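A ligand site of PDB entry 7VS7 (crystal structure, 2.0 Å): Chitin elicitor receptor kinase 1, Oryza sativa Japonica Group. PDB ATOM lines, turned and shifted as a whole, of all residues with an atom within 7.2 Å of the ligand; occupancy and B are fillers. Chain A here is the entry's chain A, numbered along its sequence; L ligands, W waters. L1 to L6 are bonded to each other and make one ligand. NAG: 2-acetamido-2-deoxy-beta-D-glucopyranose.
The backbone NH (N) of Ile 120 is in hydrogen-bond range of an oxygen (O6) of NAG L4.
O7 of NAG L5 is in hydrogen-bond range of N of Gly 90, at 3.2 Å.
The backbone carbonyl oxygen of Ile 120 sits at hydrogen-bond distance from a nitrogen (N2) of NAG L5, at 2.7 Å.
An oxygen (O3) of NAG L5 lies within hydrogen-bond range of the backbone NH (N) of Asp 122, 3.5 Å away.
An oxygen (O7) of NAG L3 sits at hydrogen-bond distance from the backbone NH (N) of Tyr 93, at 3.3 Å.
The backbone NH of Asn 119 lies within hydrogen-bond range of an oxygen (O6) of NAG L4 (3.1 Å).
OG1 of Thr 94 is in hydrogen-bond range of O7 of NAG L3 (3.0 Å).
The backbone carbonyl oxygen (O) of Ala 117 sits at hydrogen-bond distance from an oxygen (O6) of NAG L4 (2.7 Å).
O7 of NAG L3 is in hydrogen-bond range of N of Thr 94 (3.0 Å).
The backbone carbonyl oxygen (O) of Ile 92 is in hydrogen-bond range of the side-chain hydroxyl (OG) of Ser 95 (3.0 Å).
NE of Arg 89 is in salt-bridge range of OD2 of Asp 122 (3.1 Å).
The backbone carbonyl oxygen of Asp 122 sits close to the backbone NH of Ser 88 (3.5 Å).
OH of Tyr 93 lies within hydrogen-bond range of O of Tyr 115, at 2.8 Å.
The side-chain hydroxyl (OG) of Ser 95 lies within hydrogen-bond range of the side-chain amide oxygen (OE1) of Gln 91 (3.4 Å).
Met 87 touches the ligand.
O of Ser 88 touches C8 of NAG L5, at 3.3 Å.
Arg 89 touches the ligand.
O of Gln 91 touches C8 of NAG L5, at 3.6 Å.
Ile 92 touches the ligand.
OE1 of Gln 110 touches C8 of NAG L3, 3.8 Å away.
C of Asn 118 touches O6 of NAG L4, 3.2 Å away.
Of the 22 residues printed, 14 come within 4 Å of the ligand.
Water W4 lies within hydrogen-bond range of an oxygen (O3) of NAG L3, the backbone NH (N) of Tyr 93 and the backbone carbonyl oxygen (O) of Ala 117.
Water W3 lies within hydrogen-bond range of O3 of NAG L5 (2.9 Å) and OD1 of Asp 122 (3.0 Å).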
ATOM      1  N   MET A  87      -6.253  23.804 -23.446  1.00  0.00           N
ATOM      2  CA  MET A  87      -5.302  24.677 -22.794  1.00  0.00           C
ATOM      3  C   MET A  87      -5.101  25.966 -23.572  1.00  0.00           C
ATOM      4  O   MET A  87      -5.326  26.039 -24.787  1.00  0.00           O
ATOM      5  CB  MET A  87      -3.943  23.975 -22.618  1.00  0.00           C
ATOM      6  CG  MET A  87      -3.962  22.802 -21.670  1.00  0.00           C
ATOM      7  SD  MET A  87      -4.279  23.295 -19.974  1.00  0.00           S
ATOM      8  CE  MET A  87      -2.793  24.255 -19.620  1.00  0.00           C
ATOM      9  N   SER A  88      -4.677  27.003 -22.853  1.00  0.00           N
ATOM     10  CA  SER A  88      -4.091  28.190 -23.447  1.00  0.00           C
ATOM     11  C   SER A  88      -2.989  28.664 -22.507  1.00  0.00           C
ATOM     12  O   SER A  88      -2.809  28.110 -21.419  1.00  0.00           O
ATOM     13  CB  SER A  88      -5.148  29.268 -23.697  1.00  0.00           C
ATOM     14  OG  SER A  88      -5.987  29.410 -22.569  1.00  0.00           O
ATOM     15  N   ARG A  89      -2.260  29.691 -22.914  1.00  0.00           N
ATOM     16  CA  ARG A  89      -1.202  30.202 -22.063  1.00  0.00           C
ATOM     17  C   ARG A  89      -1.785  30.698 -20.740  1.00  0.00           C
ATOM     18  O   ARG A  89      -2.815  31.371 -20.716  1.00  0.00           O
ATOM     19  CB  ARG A  89      -0.457  31.333 -22.777  1.00  0.00           C
ATOM     20  CG  ARG A  89      -0.003  30.916 -24.156  1.00  0.00           C
ATOM     21  CD  ARG A  89       1.139  31.760 -24.648  1.00  0.00           C
ATOM     22  NE  ARG A  89       1.654  31.228 -25.897  1.00  0.00           N
ATOM     23  CZ  ARG A  89       2.707  31.736 -26.534  1.00  0.00           C
ATOM     24  NH1 ARG A  89       3.339  32.794 -26.027  1.00  0.00           N
ATOM     25  NH2 ARG A  89       3.125  31.190 -27.667  1.00  0.00           N
ATOM     26  N   GLY A  90      -1.142  30.304 -19.634  1.00  0.00           N
ATOM     27  CA  GLY A  90      -1.507  30.814 -18.334  1.00  0.00           C
ATOM     28  C   GLY A  90      -2.317  29.880 -17.457  1.00  0.00           C
ATOM     29  O   GLY A  90      -2.599  30.245 -16.315  1.00  0.00           O
ATOM     30  N   GLN A  91      -2.688  28.707 -17.952  1.00  0.00           N
ATOM     31  CA  GLN A  91      -3.508  27.770 -17.195  1.00  0.00           C
ATOM     32  C   GLN A  91      -2.628  26.748 -16.493  1.00  0.00           C
ATOM     33  O   GLN A  91      -1.578  26.349 -17.004  1.00  0.00           O
ATOM     34  CB  GLN A  91      -4.514  27.085 -18.113  1.00  0.00           C
ATOM     35  CG  GLN A  91      -5.593  28.029 -18.634  1.00  0.00           C
ATOM     36  CD  GLN A  91      -6.512  28.540 -17.528  1.00  0.00           C
ATOM     37  OE1 GLN A  91      -7.234  27.759 -16.884  1.00  0.00           O
ATOM     38  NE2 GLN A  91      -6.474  29.837 -17.279  1.00  0.00           N
ATOM     39  N   ILE A  92      -3.050  26.359 -15.288  1.00  0.00           N
ATOM     40  CA  ILE A  92      -2.327  25.390 -14.475  1.00  0.00           C
ATOM     41  C   ILE A  92      -3.338  24.428 -13.880  1.00  0.00           C
ATOM     42  O   ILE A  92      -4.547  24.703 -13.857  1.00  0.00           O
ATOM     43  CB  ILE A  92      -1.494  26.065 -13.352  1.00  0.00           C
ATOM     44  CG1 ILE A  92      -2.393  26.873 -12.416  1.00  0.00           C
ATOM     45  CG2 ILE A  92      -0.432  26.974 -13.938  1.00  0.00           C
ATOM     46  CD1 ILE A  92      -1.626  27.619 -11.355  1.00  0.00           C
ATOM     47  N   TYR A  93      -2.853  23.265 -13.427  1.00  0.00           N
ATOM     48  CA  TYR A  93      -3.773  22.251 -12.891  1.00  0.00           C
ATOM     49  C   TYR A  93      -4.608  22.816 -11.755  1.00  0.00           C
ATOM     50  O   TYR A  93      -5.799  22.484 -11.625  1.00  0.00           O
ATOM     51  CB  TYR A  93      -3.004  21.017 -12.406  1.00  0.00           C
ATOM     52  CG  TYR A  93      -2.521  20.088 -13.505  1.00  0.00           C
ATOM     53  CD1 TYR A  93      -3.353  19.726 -14.558  1.00  0.00           C
ATOM     54  CD2 TYR A  93      -1.230  19.585 -13.503  1.00  0.00           C
ATOM     55  CE1 TYR A  93      -2.901  18.888 -15.567  1.00  0.00           C
ATOM     56  CE2 TYR A  93      -0.772  18.739 -14.496  1.00  0.00           C
ATOM     57  CZ  TYR A  93      -1.625  18.396 -15.540  1.00  0.00           C
ATOM     58  OH  TYR A  93      -1.196  17.555 -16.541  1.00  0.00           O
ATOM     59  N   THR A  94      -3.998  23.651 -10.911  1.00  0.00           N
ATOM     60  CA  THR A  94      -4.714  24.264  -9.800  1.00  0.00           C
ATOM     61  C   THR A  94      -5.910  25.092 -10.270  1.00  0.00           C
ATOM     62  O   THR A  94      -6.987  25.021  -9.669  1.00  0.00           O
ATOM     63  CB  THR A  94      -3.745  25.130  -8.989  1.00  0.00           C
ATOM     64  OG1 THR A  94      -2.710  24.292  -8.473  1.00  0.00           O
ATOM     65  CG2 THR A  94      -4.461  25.810  -7.837  1.00  0.00           C
ATOM     66  N   SER A  95      -5.744  25.866 -11.344  1.00  0.00           N
ATOM     67  CA  SER A  95      -6.844  26.745 -11.748  1.00  0.00           C
ATOM     68  C   SER A  95      -7.939  25.972 -12.468  1.00  0.00           C
ATOM     69  O   SER A  95      -9.121  26.338 -12.374  1.00  0.00           O
ATOM     70  CB  SER A  95      -6.326  27.908 -12.608  1.00  0.00           C
ATOM     71  OG  SER A  95      -5.815  27.473 -13.861  1.00  0.00           O
ATOM     72  N   VAL A  96      -7.593  24.883 -13.157  1.00  0.00           N
ATOM     73  CA  VAL A  96      -8.611  23.986 -13.695  1.00  0.00           C
ATOM     74  C   VAL A  96      -9.401  23.355 -12.556  1.00  0.00           C
ATOM     75  O   VAL A  96     -10.638  23.389 -12.537  1.00  0.00           O
ATOM     76  CB  VAL A  96      -7.955  22.918 -14.587  1.00  0.00           C
ATOM     77  CG1 VAL A  96      -9.016  21.984 -15.142  1.00  0.00           C
ATOM     78  CG2 VAL A  96      -7.174  23.588 -15.710  1.00  0.00           C
ATOM     79  N   ALA A 106      -6.269  19.383  -7.469  1.00  0.00           N
ATOM     80  CA  ALA A 106      -5.114  19.609  -8.339  1.00  0.00           C
ATOM     81  C   ALA A 106      -4.210  18.377  -8.391  1.00  0.00           C
ATOM     82  O   ALA A 106      -3.772  17.971  -9.474  1.00  0.00           O
ATOM     83  CB  ALA A 106      -4.333  20.826  -7.860  1.00  0.00           C
ATOM     84  N   GLU A 107      -3.933  17.756  -7.235  1.00  0.00           N
ATOM     85  CA  GLU A 107      -3.051  16.587  -7.206  1.00  0.00           C
ATOM     86  C   GLU A 107      -3.624  15.438  -8.024  1.00  0.00           C
ATOM     87  O   GLU A 107      -2.876  14.740  -8.728  1.00  0.00           O
ATOM     88  CB  GLU A 107      -2.827  16.124  -5.761  1.00  0.00           C
ATOM     89  CG  GLU A 107      -2.415  17.203  -4.777  1.00  0.00           C
ATOM     90  CD  GLU A 107      -3.613  17.877  -4.095  1.00  0.00           C
ATOM     91  OE1 GLU A 107      -4.416  18.534  -4.799  1.00  0.00           O
ATOM     92  OE2 GLU A 107      -3.744  17.730  -2.852  1.00  0.00           O
ATOM     93  N   GLN A 110      -3.214  16.230 -11.725  1.00  0.00           N
ATOM     94  CA  GLN A 110      -1.831  15.910 -12.064  1.00  0.00           C
ATOM     95  C   GLN A 110      -1.637  14.415 -12.245  1.00  0.00           C
ATOM     96  O   GLN A 110      -0.985  13.982 -13.208  1.00  0.00           O
ATOM     97  CB  GLN A 110      -0.920  16.450 -10.962  1.00  0.00           C
ATOM     98  CG  GLN A 110       0.552  16.445 -11.288  1.00  0.00           C
ATOM     99  CD  GLN A 110       1.308  17.446 -10.420  1.00  0.00           C
ATOM    100  OE1 GLN A 110       0.703  18.161  -9.616  1.00  0.00           O
ATOM    101  NE2 GLN A 110       2.628  17.501 -10.574  1.00  0.00           N
ATOM    102  N   TYR A 115       0.833  15.087 -18.540  1.00  0.00           N
ATOM    103  CA  TYR A 115       1.832  16.142 -18.574  1.00  0.00           C
ATOM    104  C   TYR A 115       2.278  16.528 -17.166  1.00  0.00           C
ATOM    105  O   TYR A 115       1.451  16.592 -16.246  1.00  0.00           O
ATOM    106  CB  TYR A 115       1.305  17.399 -19.277  1.00  0.00           C
ATOM    107  CG  TYR A 115       0.910  17.204 -20.723  1.00  0.00           C
ATOM    108  CD1 TYR A 115       1.870  16.959 -21.700  1.00  0.00           C
ATOM    109  CD2 TYR A 115      -0.426  17.242 -21.107  1.00  0.00           C
ATOM    110  CE1 TYR A 115       1.507  16.774 -23.023  1.00  0.00           C
ATOM    111  CE2 TYR A 115      -0.792  17.060 -22.421  1.00  0.00           C
ATOM    112  CZ  TYR A 115       0.174  16.821 -23.377  1.00  0.00           C
ATOM    113  OH  TYR A 115      -0.181  16.637 -24.689  1.00  0.00           O
ATOM    114  N   PRO A 116       3.560  16.811 -16.965  1.00  0.00           N
ATOM    115  CA  PRO A 116       3.997  17.334 -15.675  1.00  0.00           C
ATOM    116  C   PRO A 116       3.420  18.733 -15.452  1.00  0.00           C
ATOM    117  O   PRO A 116       3.257  19.512 -16.392  1.00  0.00           O
ATOM    118  CB  PRO A 116       5.521  17.389 -15.806  1.00  0.00           C
ATOM    119  CG  PRO A 116       5.783  17.442 -17.280  1.00  0.00           C
ATOM    120  CD  PRO A 116       4.668  16.665 -17.926  1.00  0.00           C
ATOM    121  N   ALA A 117       3.116  19.032 -14.193  1.00  0.00           N
ATOM    122  CA  ALA A 117       2.472  20.292 -13.847  1.00  0.00           C
ATOM    123  C   ALA A 117       3.227  21.493 -14.399  1.00  0.00           C
ATOM    124  O   ALA A 117       2.622  22.464 -14.872  1.00  0.00           O
ATOM    125  CB  ALA A 117       2.326  20.437 -12.334  1.00  0.00           C
ATOM    126  N   ASN A 118       4.567  21.448 -14.338  1.00  0.00           N
ATOM    127  CA  ASN A 118       5.358  22.615 -14.696  1.00  0.00           C
ATOM    128  C   ASN A 118       5.681  22.704 -16.181  1.00  0.00           C
ATOM    129  O   ASN A 118       6.438  23.585 -16.583  1.00  0.00           O
ATOM    130  CB  ASN A 118       6.638  22.697 -13.836  1.00  0.00           C
ATOM    131  CG  ASN A 118       7.697  21.666 -14.222  1.00  0.00           C
ATOM    132  OD1 ASN A 118       7.584  20.943 -15.207  1.00  0.00           O
ATOM    133  ND2 ASN A 118       8.767  21.626 -13.437  1.00  0.00           N
ATOM    134  N   ASN A 119       5.112  21.820 -17.009  1.00  0.00           N
ATOM    135  CA  ASN A 119       5.343  21.923 -18.453  1.00  0.00           C
ATOM    136  C   ASN A 119       4.171  21.304 -19.223  1.00  0.00           C
ATOM    137  O   ASN A 119       4.320  20.333 -19.965  1.00  0.00           O
ATOM    138  CB  ASN A 119       6.671  21.269 -18.833  1.00  0.00           C
ATOM    139  CG  ASN A 119       7.145  21.687 -20.211  1.00  0.00           C
ATOM    140  OD1 ASN A 119       6.672  22.686 -20.765  1.00  0.00           O
ATOM    141  ND2 ASN A 119       8.057  20.926 -20.781  1.00  0.00           N
ATOM    142  N   ILE A 120       2.995  21.882 -19.066  1.00  0.00           N
ATOM    143  CA  ILE A 120       1.833  21.557 -19.887  1.00  0.00           C
ATOM    144  C   ILE A 120       1.906  22.428 -21.137  1.00  0.00           C
ATOM    145  O   ILE A 120       1.865  23.659 -21.022  1.00  0.00           O
ATOM    146  CB  ILE A 120       0.529  21.814 -19.140  1.00  0.00           C
ATOM    147  CG1 ILE A 120       0.508  21.062 -17.814  1.00  0.00           C
ATOM    148  CG2 ILE A 120      -0.666  21.460 -20.012  1.00  0.00           C
ATOM    149  CD1 ILE A 120      -0.590  21.515 -16.899  1.00  0.00           C
ATOM    150  N   PRO A 121       2.010  21.843 -22.334  1.00  0.00           N
ATOM    151  CA  PRO A 121       2.036  22.670 -23.555  1.00  0.00           C
ATOM    152  C   PRO A 121       0.767  23.507 -23.675  1.00  0.00           C
ATOM    153  O   PRO A 121      -0.332  23.072 -23.324  1.00  0.00           O
ATOM    154  CB  PRO A 121       2.134  21.643 -24.688  1.00  0.00           C
ATOM    155  CG  PRO A 121       2.624  20.390 -24.038  1.00  0.00           C
ATOM    156  CD  PRO A 121       2.078  20.405 -22.638  1.00  0.00           C
ATOM    157  N   ASP A 122       0.935  24.743 -24.169  1.00  0.00           N
ATOM    158  CA  ASP A 122      -0.188  25.685 -24.220  1.00  0.00           C
ATOM    159  C   ASP A 122      -1.259  25.290 -25.225  1.00  0.00           C
ATOM    160  O   ASP A 122      -2.368  25.840 -25.173  1.00  0.00           O
ATOM    161  CB  ASP A 122       0.326  27.096 -24.531  1.00  0.00           C
ATOM    162  CG  ASP A 122       1.086  27.171 -25.853  1.00  0.00           C
ATOM    163  OD1 ASP A 122       1.709  26.162 -26.241  1.00  0.00           O
ATOM    164  OD2 ASP A 122       1.069  28.256 -26.494  1.00  0.00           O
ATOM    165  N   THR A 123      -0.952  24.367 -26.136  1.00  0.00           N
ATOM    166  CA  THR A 123      -1.908  23.900 -27.144  1.00  0.00           C
ATOM    167  C   THR A 123      -2.526  22.546 -26.800  1.00  0.00           C
ATOM    168  O   THR A 123      -3.335  22.042 -27.601  1.00  0.00           O
ATOM    169  CB  THR A 123      -1.208  23.818 -28.497  1.00  0.00           C
ATOM    170  OG1 THR A 123      -0.033  23.008 -28.364  1.00  0.00           O
ATOM    171  CG2 THR A 123      -0.799  25.217 -28.967  1.00  0.00           C
HETATM  172  C1  NAG L   1      -2.519  28.585  -0.114  1.00  0.00           C
HETATM  173  C2  NAG L   1      -2.127  27.185  -0.658  1.00  0.00           C
HETATM  174  C3  NAG L   1      -1.300  27.233  -1.977  1.00  0.00           C
HETATM  175  C4  NAG L   1      -1.605  28.425  -2.881  1.00  0.00           C
HETATM  176  C5  NAG L   1      -1.839  29.673  -2.042  1.00  0.00           C
HETATM  177  C6  NAG L   1      -2.196  30.898  -2.850  1.00  0.00           C
HETATM  178  C7  NAG L   1      -0.264  26.587   0.967  1.00  0.00           C
HETATM  179  C8  NAG L   1       0.499  27.848   0.611  1.00  0.00           C
HETATM  180  N2  NAG L   1      -1.454  26.366   0.350  1.00  0.00           N
HETATM  181  O1  NAG L   1      -3.567  28.444   0.802  1.00  0.00           O
HETATM  182  O3  NAG L   1      -1.530  26.028  -2.702  1.00  0.00           O
HETATM  183  O4  NAG L   1      -0.472  28.660  -3.705  1.00  0.00           O
HETATM  184  O5  NAG L   1      -2.929  29.415  -1.157  1.00  0.00           O
HETATM  185  O6  NAG L   1      -3.262  30.642  -3.753  1.00  0.00           O
HETATM  186  O7  NAG L   1       0.180  25.800   1.795  1.00  0.00           O
HETATM  187  C1  NAG L   2      -0.506  28.086  -5.044  1.00  0.00           C
HETATM  188  C2  NAG L   2       0.525  28.866  -5.861  1.00  0.00           C
HETATM  189  C3  NAG L   2       0.601  28.314  -7.282  1.00  0.00           C
HETATM  190  C4  NAG L   2       0.816  26.807  -7.281  1.00  0.00           C
HETATM  191  C5  NAG L   2      -0.244  26.140  -6.403  1.00  0.00           C
HETATM  192  C6  NAG L   2      -0.053  24.650  -6.261  1.00  0.00           C
HETATM  193  C7  NAG L   2       1.004  31.222  -5.321  1.00  0.00           C
HETATM  194  C8  NAG L   2       0.519  32.633  -5.431  1.00  0.00           C
HETATM  195  N2  NAG L   2       0.214  30.286  -5.872  1.00  0.00           N
HETATM  196  O3  NAG L   2       1.675  28.957  -7.953  1.00  0.00           O
HETATM  197  O4  NAG L   2       0.628  26.289  -8.597  1.00  0.00           O
HETATM  198  O5  NAG L   2      -0.199  26.696  -5.077  1.00  0.00           O
HETATM  199  O6  NAG L   2       1.186  24.358  -5.630  1.00  0.00           O
HETATM  200  O7  NAG L   2       2.067  30.937  -4.773  1.00  0.00           O
HETATM  201  C1  NAG L   3       1.812  26.035  -9.361  1.00  0.00           C
HETATM  202  C2  NAG L   3       1.469  25.049 -10.505  1.00  0.00           C
HETATM  203  C3  NAG L   3       2.626  24.918 -11.482  1.00  0.00           C
HETATM  204  C4  NAG L   3       3.076  26.291 -11.967  1.00  0.00           C
HETATM  205  C5  NAG L   3       3.428  27.137 -10.748  1.00  0.00           C
HETATM  206  C6  NAG L   3       3.846  28.552 -11.091  1.00  0.00           C
HETATM  207  C7  NAG L   3      -0.099  23.196 -10.168  1.00  0.00           C
HETATM  208  C8  NAG L   3      -0.322  21.842  -9.545  1.00  0.00           C
HETATM  209  N2  NAG L   3       1.111  23.744  -9.971  1.00  0.00           N
HETATM  210  O3  NAG L   3       2.229  24.146 -12.608  1.00  0.00           O
HETATM  211  O4  NAG L   3       4.212  26.133 -12.809  1.00  0.00           O
HETATM  212  O5  NAG L   3       2.272  27.247  -9.903  1.00  0.00           O
HETATM  213  O6  NAG L   3       2.915  29.164 -11.969  1.00  0.00           O
HETATM  214  O7  NAG L   3      -0.966  23.760 -10.808  1.00  0.00           O
HETATM  215  C1  NAG L   4       3.974  26.635 -14.140  1.00  0.00           C
HETATM  216  C2  NAG L   4       5.321  26.913 -14.761  1.00  0.00           C
HETATM  217  C3  NAG L   4       5.142  27.436 -16.185  1.00  0.00           C
HETATM  218  C4  NAG L   4       4.281  26.470 -16.991  1.00  0.00           C
HETATM  219  C5  NAG L   4       2.981  26.176 -16.246  1.00  0.00           C
HETATM  220  C6  NAG L   4       2.148  25.121 -16.937  1.00  0.00           C
HETATM  221  C7  NAG L   4       7.071  27.472 -13.107  1.00  0.00           C
HETATM  222  C8  NAG L   4       7.720  28.568 -12.329  1.00  0.00           C
HETATM  223  N2  NAG L   4       6.090  27.852 -13.943  1.00  0.00           N
HETATM  224  O3  NAG L   4       6.425  27.581 -16.803  1.00  0.00           O
HETATM  225  O4  NAG L   4       3.894  27.062 -18.224  1.00  0.00           O
HETATM  226  O5  NAG L   4       3.280  25.684 -14.937  1.00  0.00           O
HETATM  227  O6  NAG L   4       2.887  23.917 -17.098  1.00  0.00           O
HETATM  228  O7  NAG L   4       7.420  26.307 -13.007  1.00  0.00           O
HETATM  229  C1  NAG L   5       4.447  26.411 -19.377  1.00  0.00           C
HETATM  230  C2  NAG L   5       3.620  26.798 -20.618  1.00  0.00           C
HETATM  231  C3  NAG L   5       4.273  26.248 -21.885  1.00  0.00           C
HETATM  232  C4  NAG L   5       5.738  26.654 -21.973  1.00  0.00           C
HETATM  233  C5  NAG L   5       6.439  26.216 -20.687  1.00  0.00           C
HETATM  234  C6  NAG L   5       7.895  26.614 -20.633  1.00  0.00           C
HETATM  235  C7  NAG L   5       1.196  27.132 -20.374  1.00  0.00           C
HETATM  236  C8  NAG L   5      -0.141  26.466 -20.294  1.00  0.00           C
HETATM  237  N2  NAG L   5       2.253  26.322 -20.505  1.00  0.00           N
HETATM  238  O3  NAG L   5       3.555  26.705 -23.020  1.00  0.00           O
HETATM  239  O4  NAG L   5       6.339  25.933 -23.037  1.00  0.00           O
HETATM  240  O5  NAG L   5       5.800  26.817 -19.555  1.00  0.00           O
HETATM  241  O6  NAG L   5       8.051  27.994 -20.303  1.00  0.00           O
HETATM  242  O7  NAG L   5       1.323  28.350 -20.306  1.00  0.00           O
HETATM  243  C1  NAG L   6       6.921  26.704 -24.098  1.00  0.00           C
HETATM  244  C2  NAG L   6       7.944  25.793 -24.818  1.00  0.00           C
HETATM  245  C3  NAG L   6       8.520  26.488 -26.059  1.00  0.00           C
HETATM  246  C4  NAG L   6       7.411  27.036 -26.940  1.00  0.00           C
HETATM  247  C5  NAG L   6       6.497  27.941 -26.119  1.00  0.00           C
HETATM  248  C6  NAG L   6       5.331  28.503 -26.898  1.00  0.00           C
HETATM  249  C7  NAG L   6       9.225  24.130 -23.545  1.00  0.00           C
HETATM  250  C8  NAG L   6      10.379  23.904 -22.598  1.00  0.00           C
HETATM  251  N2  NAG L   6       9.007  25.393 -23.913  1.00  0.00           N
HETATM  252  O3  NAG L   6       9.303  25.554 -26.799  1.00  0.00           O
HETATM  253  O4  NAG L   6       7.964  27.787 -28.021  1.00  0.00           O
HETATM  254  O5  NAG L   6       5.951  27.179 -25.032  1.00  0.00           O
HETATM  255  O6  NAG L   6       4.857  27.583 -27.866  1.00  0.00           O
HETATM  256  O7  NAG L   6       8.534  23.205 -23.949  1.00  0.00           O
HETATM  257  O   HOH W   1       3.305  22.250  -8.709  1.00  0.00           O
HETATM  258  O   HOH W   2       2.565  30.623 -21.311  1.00  0.00           O
HETATM  259  O   HOH W   3       4.205  24.845 -25.099  1.00  0.00           O
HETATM  260  O   HOH W   4      -0.047  22.992 -13.688  1.00  0.00           O
